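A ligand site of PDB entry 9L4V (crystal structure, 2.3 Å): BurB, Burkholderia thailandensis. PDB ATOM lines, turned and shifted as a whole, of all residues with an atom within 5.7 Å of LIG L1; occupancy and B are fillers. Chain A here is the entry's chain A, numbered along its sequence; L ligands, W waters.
N of His 93 lies within hydrogen-bond range of N3 of LIG L1, 2.9 Å away. The backbone carbonyl oxygen (O) of His 93 lies within hydrogen-bond range of a nitrogen (N4) of LIG L1 (2.7 Å). An oxygen (O4) of LIG L1 sits at hydrogen-bond distance from the guanidinium group of Arg 133, at 2.8 Å. The backbone NH (N) of Ala 44 sits at hydrogen-bond distance from an oxygen (O1) of LIG L1, 2.7 Å away. The backbone NH (N) of His 138 is in hydrogen-bond range of a nitrogen (N5) of LIG L1 (2.9 Å). The backbone carbonyl oxygen of Ala 44 lies within hydrogen-bond range of a nitrogen (N1) of LIG L1 (2.7 Å). O of Arg 42 lies within hydrogen-bond range of N1 of LIG L1 (3.0 Å). The side-chain sulfur (SG) of Cys 137 sits at hydrogen-bond distance from a nitrogen (N4) of LIG L1, 3.6 Å away.
The side-chain hydroxyl (OH) of Tyr 124 lies within hydrogen-bond range of the backbone carbonyl oxygen (O) of Leu 91, at 2.6 Å. A ring nitrogen (ND1) of His 93 lies within hydrogen-bond range of the backbone NH of Tyr 124 (3.1 Å). The side-chain sulfur (SG) of Cys 137 lies within hydrogen-bond range of the backbone NH (N) of Cys 139, 3.4 Å away. ND1 of His 72 lies within hydrogen-bond range of O of Gly 89 (3.4 Å).
C of Gly 43 touches O1 of LIG L1 (3.6 Å). O of Leu 71 touches C5 of LIG L1, 2.9 Å away. ND1 of His 72 touches C5 of LIG L1 (3.0 Å). Gly 89 touches LIG L1 (O to C4, 3.2 Å). Leu 90 touches LIG L1. Leu 92 touches LIG L1 (CD2 to C11, 3.7 Å). Tyr 124 touches LIG L1 (OH to C6, 3.3 Å). Phe 135 touches LIG L1. O of Glu 136 touches C14 of LIG L1, 3.4 Å away. Cys 139 touches LIG L1 (N to N4, 3.98 Å). 16 residues have an atom within 4 Å of LIG L1: Arg 42, Gly 43, Ala 44, Leu 71, His 72, Gly 89, Leu 90, Leu 92, His 93, Tyr 124, Arg 133, Phe 135, Glu 136, Cys 137, His 138 and Cys 139.
Water W2 lies within hydrogen-bond range of O1 of LG2 L2 (2.5 Å), O4 of LIG L1 (2.7 Å) and O of Arg 133 (2.9 Å). Water W4 bridges O5 of LIG L1 (3.4 Å) and N of Gly 43 (3.5 Å). Water W1 lies within hydrogen-bond range of O of His 93 (2.6 Å), NH1 of Arg 42 (3.0 Å) and N4 of LIG L1 (3.4 Å).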
ATOM      1  N   GLN A  37      25.398 -19.749 -26.313  1.00  0.00           N
ATOM      2  CA  GLN A  37      24.960 -19.563 -24.937  1.00  0.00           C
ATOM      3  C   GLN A  37      25.694 -18.367 -24.349  1.00  0.00           C
ATOM      4  O   GLN A  37      26.930 -18.385 -24.257  1.00  0.00           O
ATOM      5  CB  GLN A  37      25.234 -20.799 -24.092  1.00  0.00           C
ATOM      6  CG  GLN A  37      24.142 -21.845 -24.148  1.00  0.00           C
ATOM      7  CD  GLN A  37      22.848 -21.395 -23.495  1.00  0.00           C
ATOM      8  OE1 GLN A  37      21.774 -21.765 -23.949  1.00  0.00           O
ATOM      9  NE2 GLN A  37      22.942 -20.579 -22.452  1.00  0.00           N
ATOM     10  N   GLY A  41      23.895 -14.508 -18.151  1.00  0.00           N
ATOM     11  CA  GLY A  41      22.533 -14.665 -17.673  1.00  0.00           C
ATOM     12  C   GLY A  41      21.422 -14.340 -18.656  1.00  0.00           C
ATOM     13  O   GLY A  41      20.273 -14.174 -18.243  1.00  0.00           O
ATOM     14  N   ARG A  42      21.729 -14.264 -19.957  1.00  0.00           N
ATOM     15  CA  ARG A  42      20.707 -14.001 -20.969  1.00  0.00           C
ATOM     16  C   ARG A  42      20.278 -15.260 -21.715  1.00  0.00           C
ATOM     17  O   ARG A  42      19.481 -15.173 -22.660  1.00  0.00           O
ATOM     18  CB  ARG A  42      21.195 -12.932 -21.956  1.00  0.00           C
ATOM     19  CG  ARG A  42      21.307 -11.547 -21.337  1.00  0.00           C
ATOM     20  CD  ARG A  42      21.936 -10.560 -22.323  1.00  0.00           C
ATOM     21  NE  ARG A  42      23.293 -10.933 -22.699  1.00  0.00           N
ATOM     22  CZ  ARG A  42      23.941 -10.470 -23.761  1.00  0.00           C
ATOM     23  NH1 ARG A  42      23.368  -9.628 -24.613  1.00  0.00           N
ATOM     24  NH2 ARG A  42      25.189 -10.861 -23.981  1.00  0.00           N
ATOM     25  N   GLY A  43      20.764 -16.433 -21.314  1.00  0.00           N
ATOM     26  CA  GLY A  43      20.456 -17.652 -22.032  1.00  0.00           C
ATOM     27  C   GLY A  43      21.098 -17.634 -23.410  1.00  0.00           C
ATOM     28  O   GLY A  43      22.080 -16.935 -23.677  1.00  0.00           O
ATOM     29  N   ALA A  44      20.516 -18.421 -24.313  1.00  0.00           N
ATOM     30  CA  ALA A  44      21.065 -18.462 -25.656  1.00  0.00           C
ATOM     31  C   ALA A  44      20.599 -17.250 -26.460  1.00  0.00           C
ATOM     32  O   ALA A  44      19.574 -16.624 -26.162  1.00  0.00           O
ATOM     33  CB  ALA A  44      20.651 -19.767 -26.342  1.00  0.00           C
ATOM     34  N   GLY A  45      21.374 -16.919 -27.508  1.00  0.00           N
ATOM     35  CA  GLY A  45      21.015 -15.805 -28.363  1.00  0.00           C
ATOM     36  C   GLY A  45      21.724 -15.834 -29.696  1.00  0.00           C
ATOM     37  O   GLY A  45      22.676 -16.585 -29.913  1.00  0.00           O
ATOM     38  N   LEU A  71       7.251 -18.189 -25.692  1.00  0.00           N
ATOM     39  CA  LEU A  71       8.557 -17.600 -25.412  1.00  0.00           C
ATOM     40  C   LEU A  71       9.324 -17.290 -26.700  1.00  0.00           C
ATOM     41  O   LEU A  71       9.993 -16.261 -26.813  1.00  0.00           O
ATOM     42  CB  LEU A  71       9.373 -18.501 -24.477  1.00  0.00           C
ATOM     43  CG  LEU A  71      10.764 -17.982 -24.074  1.00  0.00           C
ATOM     44  CD1 LEU A  71      10.687 -16.732 -23.196  1.00  0.00           C
ATOM     45  CD2 LEU A  71      11.648 -19.069 -23.406  1.00  0.00           C
ATOM     46  N   HIS A  72       9.177 -18.139 -27.725  1.00  0.00           N
ATOM     47  CA  HIS A  72       9.875 -17.976 -28.996  1.00  0.00           C
ATOM     48  C   HIS A  72       8.966 -17.497 -30.126  1.00  0.00           C
ATOM     49  O   HIS A  72       9.281 -17.705 -31.308  1.00  0.00           O
ATOM     50  CB  HIS A  72      10.565 -19.294 -29.383  1.00  0.00           C
ATOM     51  CG  HIS A  72      11.637 -19.721 -28.413  1.00  0.00           C
ATOM     52  ND1 HIS A  72      12.565 -18.848 -27.897  1.00  0.00           N
ATOM     53  CD2 HIS A  72      11.903 -20.926 -27.858  1.00  0.00           C
ATOM     54  CE1 HIS A  72      13.388 -19.501 -27.082  1.00  0.00           C
ATOM     55  NE2 HIS A  72      13.003 -20.773 -27.049  1.00  0.00           N
ATOM     56  N   GLY A  89      13.021 -15.766 -32.776  1.00  0.00           N
ATOM     57  CA  GLY A  89      12.703 -15.974 -31.367  1.00  0.00           C
ATOM     58  C   GLY A  89      13.916 -16.107 -30.455  1.00  0.00           C
ATOM     59  O   GLY A  89      13.793 -16.002 -29.223  1.00  0.00           O
ATOM     60  N   LEU A  90      15.106 -16.316 -31.022  1.00  0.00           N
ATOM     61  CA  LEU A  90      16.312 -16.369 -30.217  1.00  0.00           C
ATOM     62  C   LEU A  90      17.053 -15.036 -30.212  1.00  0.00           C
ATOM     63  O   LEU A  90      18.175 -14.969 -29.700  1.00  0.00           O
ATOM     64  CB  LEU A  90      17.228 -17.488 -30.702  1.00  0.00           C
ATOM     65  CG  LEU A  90      16.518 -18.845 -30.840  1.00  0.00           C
ATOM     66  CD1 LEU A  90      17.477 -19.915 -31.358  1.00  0.00           C
ATOM     67  CD2 LEU A  90      15.882 -19.261 -29.504  1.00  0.00           C
ATOM     68  N   LEU A  91      16.460 -13.976 -30.758  1.00  0.00           N
ATOM     69  CA  LEU A  91      17.055 -12.645 -30.628  1.00  0.00           C
ATOM     70  C   LEU A  91      16.885 -12.143 -29.211  1.00  0.00           C
ATOM     71  O   LEU A  91      15.771 -12.153 -28.671  1.00  0.00           O
ATOM     72  CB  LEU A  91      16.403 -11.666 -31.596  1.00  0.00           C
ATOM     73  CG  LEU A  91      16.659 -11.908 -33.067  1.00  0.00           C
ATOM     74  CD1 LEU A  91      15.685 -11.035 -33.879  1.00  0.00           C
ATOM     75  CD2 LEU A  91      18.118 -11.577 -33.404  1.00  0.00           C
ATOM     76  N   LEU A  92      17.989 -11.692 -28.596  1.00  0.00           N
ATOM     77  CA  LEU A  92      17.951 -11.212 -27.219  1.00  0.00           C
ATOM     78  C   LEU A  92      17.447  -9.785 -27.196  1.00  0.00           C
ATOM     79  O   LEU A  92      17.428  -9.087 -28.209  1.00  0.00           O
ATOM     80  CB  LEU A  92      19.338 -11.260 -26.588  1.00  0.00           C
ATOM     81  CG  LEU A  92      19.982 -12.649 -26.536  1.00  0.00           C
ATOM     82  CD1 LEU A  92      21.433 -12.535 -26.067  1.00  0.00           C
ATOM     83  CD2 LEU A  92      19.147 -13.593 -25.636  1.00  0.00           C
ATOM     84  N   HIS A  93      17.071  -9.341 -25.999  1.00  0.00           N
ATOM     85  CA  HIS A  93      16.564  -7.987 -25.824  1.00  0.00           C
ATOM     86  C   HIS A  93      17.711  -7.050 -25.479  1.00  0.00           C
ATOM     87  O   HIS A  93      18.653  -7.420 -24.775  1.00  0.00           O
ATOM     88  CB  HIS A  93      15.526  -7.915 -24.694  1.00  0.00           C
ATOM     89  CG  HIS A  93      15.236  -6.507 -24.257  1.00  0.00           C
ATOM     90  ND1 HIS A  93      14.399  -5.672 -24.966  1.00  0.00           N
ATOM     91  CD2 HIS A  93      15.721  -5.768 -23.234  1.00  0.00           C
ATOM     92  CE1 HIS A  93      14.349  -4.496 -24.380  1.00  0.00           C
ATOM     93  NE2 HIS A  93      15.145  -4.526 -23.325  1.00  0.00           N
ATOM     94  N   SER A  94      17.601  -5.811 -25.962  1.00  0.00           N
ATOM     95  CA  SER A  94      18.413  -4.736 -25.425  1.00  0.00           C
ATOM     96  C   SER A  94      17.570  -3.471 -25.404  1.00  0.00           C
ATOM     97  O   SER A  94      16.750  -3.230 -26.303  1.00  0.00           O
ATOM     98  CB  SER A  94      19.678  -4.456 -26.216  1.00  0.00           C
ATOM     99  OG  SER A  94      20.181  -3.178 -25.879  1.00  0.00           O
ATOM    100  N   TYR A 124      12.371  -5.659 -27.369  1.00  0.00           N
ATOM    101  CA  TYR A 124      11.162  -6.503 -27.367  1.00  0.00           C
ATOM    102  C   TYR A 124       9.894  -5.662 -27.346  1.00  0.00           C
ATOM    103  O   TYR A 124       8.870  -6.067 -27.898  1.00  0.00           O
ATOM    104  CB  TYR A 124      11.155  -7.444 -26.161  1.00  0.00           C
ATOM    105  CG  TYR A 124      12.098  -8.637 -26.234  1.00  0.00           C
ATOM    106  CD1 TYR A 124      12.994  -8.797 -27.283  1.00  0.00           C
ATOM    107  CD2 TYR A 124      12.097  -9.591 -25.221  1.00  0.00           C
ATOM    108  CE1 TYR A 124      13.866  -9.878 -27.326  1.00  0.00           C
ATOM    109  CE2 TYR A 124      12.956 -10.678 -25.262  1.00  0.00           C
ATOM    110  CZ  TYR A 124      13.840 -10.821 -26.303  1.00  0.00           C
ATOM    111  OH  TYR A 124      14.668 -11.920 -26.330  1.00  0.00           O
ATOM    112  N   ARG A 133       6.986 -13.851 -20.635  1.00  0.00           N
ATOM    113  CA  ARG A 133       7.471 -13.676 -19.284  1.00  0.00           C
ATOM    114  C   ARG A 133       8.273 -12.392 -19.226  1.00  0.00           C
ATOM    115  O   ARG A 133       8.949 -12.014 -20.205  1.00  0.00           O
ATOM    116  CB  ARG A 133       8.323 -14.880 -18.823  1.00  0.00           C
ATOM    117  CG  ARG A 133       9.702 -14.960 -19.504  1.00  0.00           C
ATOM    118  CD  ARG A 133      10.270 -16.394 -19.536  1.00  0.00           C
ATOM    119  NE  ARG A 133      11.695 -16.402 -19.879  1.00  0.00           N
ATOM    120  CZ  ARG A 133      12.453 -17.488 -19.961  1.00  0.00           C
ATOM    121  NH1 ARG A 133      11.972 -18.683 -19.668  1.00  0.00           N
ATOM    122  NH2 ARG A 133      13.719 -17.378 -20.354  1.00  0.00           N
ATOM    123  N   GLN A 134       8.179 -11.705 -18.104  1.00  0.00           N
ATOM    124  CA  GLN A 134       9.002 -10.546 -17.808  1.00  0.00           C
ATOM    125  C   GLN A 134      10.329 -11.009 -17.192  1.00  0.00           C
ATOM    126  O   GLN A 134      10.444 -12.125 -16.665  1.00  0.00           O
ATOM    127  CB  GLN A 134       8.259  -9.590 -16.860  1.00  0.00           C
ATOM    128  CG  GLN A 134       6.773  -9.412 -17.221  1.00  0.00           C
ATOM    129  CD  GLN A 134       6.039  -8.379 -16.347  1.00  0.00           C
ATOM    130  OE1 GLN A 134       6.644  -7.726 -15.485  1.00  0.00           O
ATOM    131  NE2 GLN A 134       4.740  -8.218 -16.579  1.00  0.00           N
ATOM    132  N   PHE A 135      11.346 -10.161 -17.292  1.00  0.00           N
ATOM    133  CA  PHE A 135      12.666 -10.544 -16.819  1.00  0.00           C
ATOM    134  C   PHE A 135      13.490  -9.309 -16.516  1.00  0.00           C
ATOM    135  O   PHE A 135      13.273  -8.236 -17.095  1.00  0.00           O
ATOM    136  CB  PHE A 135      13.396 -11.400 -17.861  1.00  0.00           C
ATOM    137  CG  PHE A 135      13.542 -10.742 -19.214  1.00  0.00           C
ATOM    138  CD1 PHE A 135      14.650  -9.959 -19.502  1.00  0.00           C
ATOM    139  CD2 PHE A 135      12.577 -10.931 -20.199  1.00  0.00           C
ATOM    140  CE1 PHE A 135      14.792  -9.366 -20.776  1.00  0.00           C
ATOM    141  CE2 PHE A 135      12.703 -10.343 -21.448  1.00  0.00           C
ATOM    142  CZ  PHE A 135      13.819  -9.568 -21.745  1.00  0.00           C
ATOM    143  N   GLU A 136      14.434  -9.466 -15.602  1.00  0.00           N
ATOM    144  CA  GLU A 136      15.375  -8.410 -15.314  1.00  0.00           C
ATOM    145  C   GLU A 136      16.410  -8.353 -16.428  1.00  0.00           C
ATOM    146  O   GLU A 136      16.891  -9.392 -16.909  1.00  0.00           O
ATOM    147  CB  GLU A 136      16.025  -8.610 -13.932  1.00  0.00           C
ATOM    148  CG  GLU A 136      17.436  -9.165 -13.939  1.00  0.00           C
ATOM    149  CD  GLU A 136      18.086  -9.202 -12.544  1.00  0.00           C
ATOM    150  OE1 GLU A 136      18.492  -8.132 -12.028  1.00  0.00           O
ATOM    151  OE2 GLU A 136      18.214 -10.312 -11.983  1.00  0.00           O
ATOM    152  N   CYS A 137      16.752  -7.143 -16.843  1.00  0.00           N
ATOM    153  CA  CYS A 137      17.508  -6.943 -18.055  1.00  0.00           C
ATOM    154  C   CYS A 137      19.002  -6.894 -17.781  1.00  0.00           C
ATOM    155  O   CYS A 137      19.456  -6.161 -16.889  1.00  0.00           O
ATOM    156  CB  CYS A 137      17.090  -5.654 -18.738  1.00  0.00           C
ATOM    157  SG  CYS A 137      17.849  -5.497 -20.335  1.00  0.00           S
ATOM    158  N   HIS A 138      19.770  -7.629 -18.575  1.00  0.00           N
ATOM    159  CA  HIS A 138      21.226  -7.633 -18.484  1.00  0.00           C
ATOM    160  C   HIS A 138      21.881  -7.021 -19.712  1.00  0.00           C
ATOM    161  O   HIS A 138      23.001  -7.393 -20.071  1.00  0.00           O
ATOM    162  CB  HIS A 138      21.731  -9.063 -18.276  1.00  0.00           C
ATOM    163  CG  HIS A 138      21.219  -9.712 -17.025  1.00  0.00           C
ATOM    164  ND1 HIS A 138      21.305  -9.110 -15.794  1.00  0.00           N
ATOM    165  CD2 HIS A 138      20.607 -10.899 -16.827  1.00  0.00           C
ATOM    166  CE1 HIS A 138      20.770  -9.908 -14.884  1.00  0.00           C
ATOM    167  NE2 HIS A 138      20.342 -11.001 -15.480  1.00  0.00           N
ATOM    168  N   CYS A 139      21.209  -6.062 -20.358  1.00  0.00           N
ATOM    169  CA  CYS A 139      21.753  -5.529 -21.604  1.00  0.00           C
ATOM    170  C   CYS A 139      22.935  -4.592 -21.358  1.00  0.00           C
ATOM    171  O   CYS A 139      23.721  -4.361 -22.276  1.00  0.00           O
ATOM    172  CB  CYS A 139      20.678  -4.796 -22.430  1.00  0.00           C
ATOM    173  SG  CYS A 139      20.254  -3.073 -21.945  1.00  0.00           S
HETATM  174  N1  LIG L   1      17.546 -16.690 -24.320  1.00  0.00           N
HETATM  175  C1  LIG L   1      16.447 -17.368 -24.985  1.00  0.00           C
HETATM  176  C2  LIG L   1      16.802 -18.790 -24.970  1.00  0.00           C
HETATM  177  O1  LIG L   1      17.853 -18.954 -24.317  1.00  0.00           O
HETATM  178  O2  LIG L   1      16.095 -19.649 -25.523  1.00  0.00           O
HETATM  179  C3  LIG L   1      16.136 -16.769 -26.381  1.00  0.00           C
HETATM  180  C4  LIG L   1      15.304 -15.482 -26.494  1.00  0.00           C
HETATM  181  S1  LIG L   1      14.060 -15.757 -25.434  1.00  0.00           S
HETATM  182  C5  LIG L   1      12.853 -16.460 -26.187  1.00  0.00           C
HETATM  183  C6  LIG L   1      13.562 -14.484 -24.483  1.00  0.00           C
HETATM  184  C7  LIG L   1      14.187 -14.672 -23.091  1.00  0.00           C
HETATM  185  O3  LIG L   1      15.606 -14.489 -23.149  1.00  0.00           O
HETATM  186  C8  LIG L   1      13.695 -13.739 -22.022  1.00  0.00           C
HETATM  187  O4  LIG L   1      12.502 -14.223 -21.440  1.00  0.00           O
HETATM  188  C9  LIG L   1      14.896 -13.735 -21.086  1.00  0.00           C
HETATM  189  O5  LIG L   1      14.933 -14.828 -20.167  1.00  0.00           O
HETATM  190  C10 LIG L   1      16.099 -13.895 -21.997  1.00  0.00           C
HETATM  191  N2  LIG L   1      16.641 -12.578 -22.318  1.00  0.00           N
HETATM  192  C11 LIG L   1      16.591 -11.995 -23.488  1.00  0.00           C
HETATM  193  N3  LIG L   1      17.172 -10.814 -23.464  1.00  0.00           N
HETATM  194  C12 LIG L   1      17.625 -10.613 -22.261  1.00  0.00           C
HETATM  195  C13 LIG L   1      18.329  -9.546 -21.577  1.00  0.00           C
HETATM  196  N4  LIG L   1      18.660  -8.466 -22.237  1.00  0.00           N
HETATM  197  N5  LIG L   1      18.628  -9.697 -20.265  1.00  0.00           N
HETATM  198  C14 LIG L   1      18.282 -10.804 -19.622  1.00  0.00           C
HETATM  199  N6  LIG L   1      17.634 -11.824 -20.197  1.00  0.00           N
HETATM  200  C15 LIG L   1      17.275 -11.783 -21.489  1.00  0.00           C
HETATM  201  C1  LG2 L   2      12.213 -13.629 -27.608  1.00  0.00           C
HETATM  202  S1  LG2 L   2      11.227 -12.961 -28.938  1.00  0.00           S
HETATM  203  C2  LG2 L   2      12.589 -11.966 -29.618  1.00  0.00           C
HETATM  204  C3  LG2 L   2      10.500 -11.744 -27.809  1.00  0.00           C
HETATM  205  C4  LG2 L   2       9.010 -12.025 -27.565  1.00  0.00           C
HETATM  206  C5  LG2 L   2       8.688 -13.360 -26.875  1.00  0.00           C
HETATM  207  N1  LG2 L   2       7.289 -13.714 -27.063  1.00  0.00           N
HETATM  208  C6  LG2 L   2       8.978 -13.271 -25.390  1.00  0.00           C
HETATM  209  O1  LG2 L   2      10.203 -12.970 -24.939  1.00  0.00           O
HETATM  210  O2  LG2 L   2       8.086 -13.474 -24.595  1.00  0.00           O
HETATM  211  O   HOH W   1      21.216  -7.628 -24.331  1.00  0.00           O
HETATM  212  O   HOH W   2      10.564 -12.749 -22.515  1.00  0.00           O
HETATM  213  O   HOH W   3      17.103 -17.619 -21.462  1.00  0.00           O
HETATM  214  O   HOH W   4      17.852 -16.429 -19.445  1.00  0.00           O
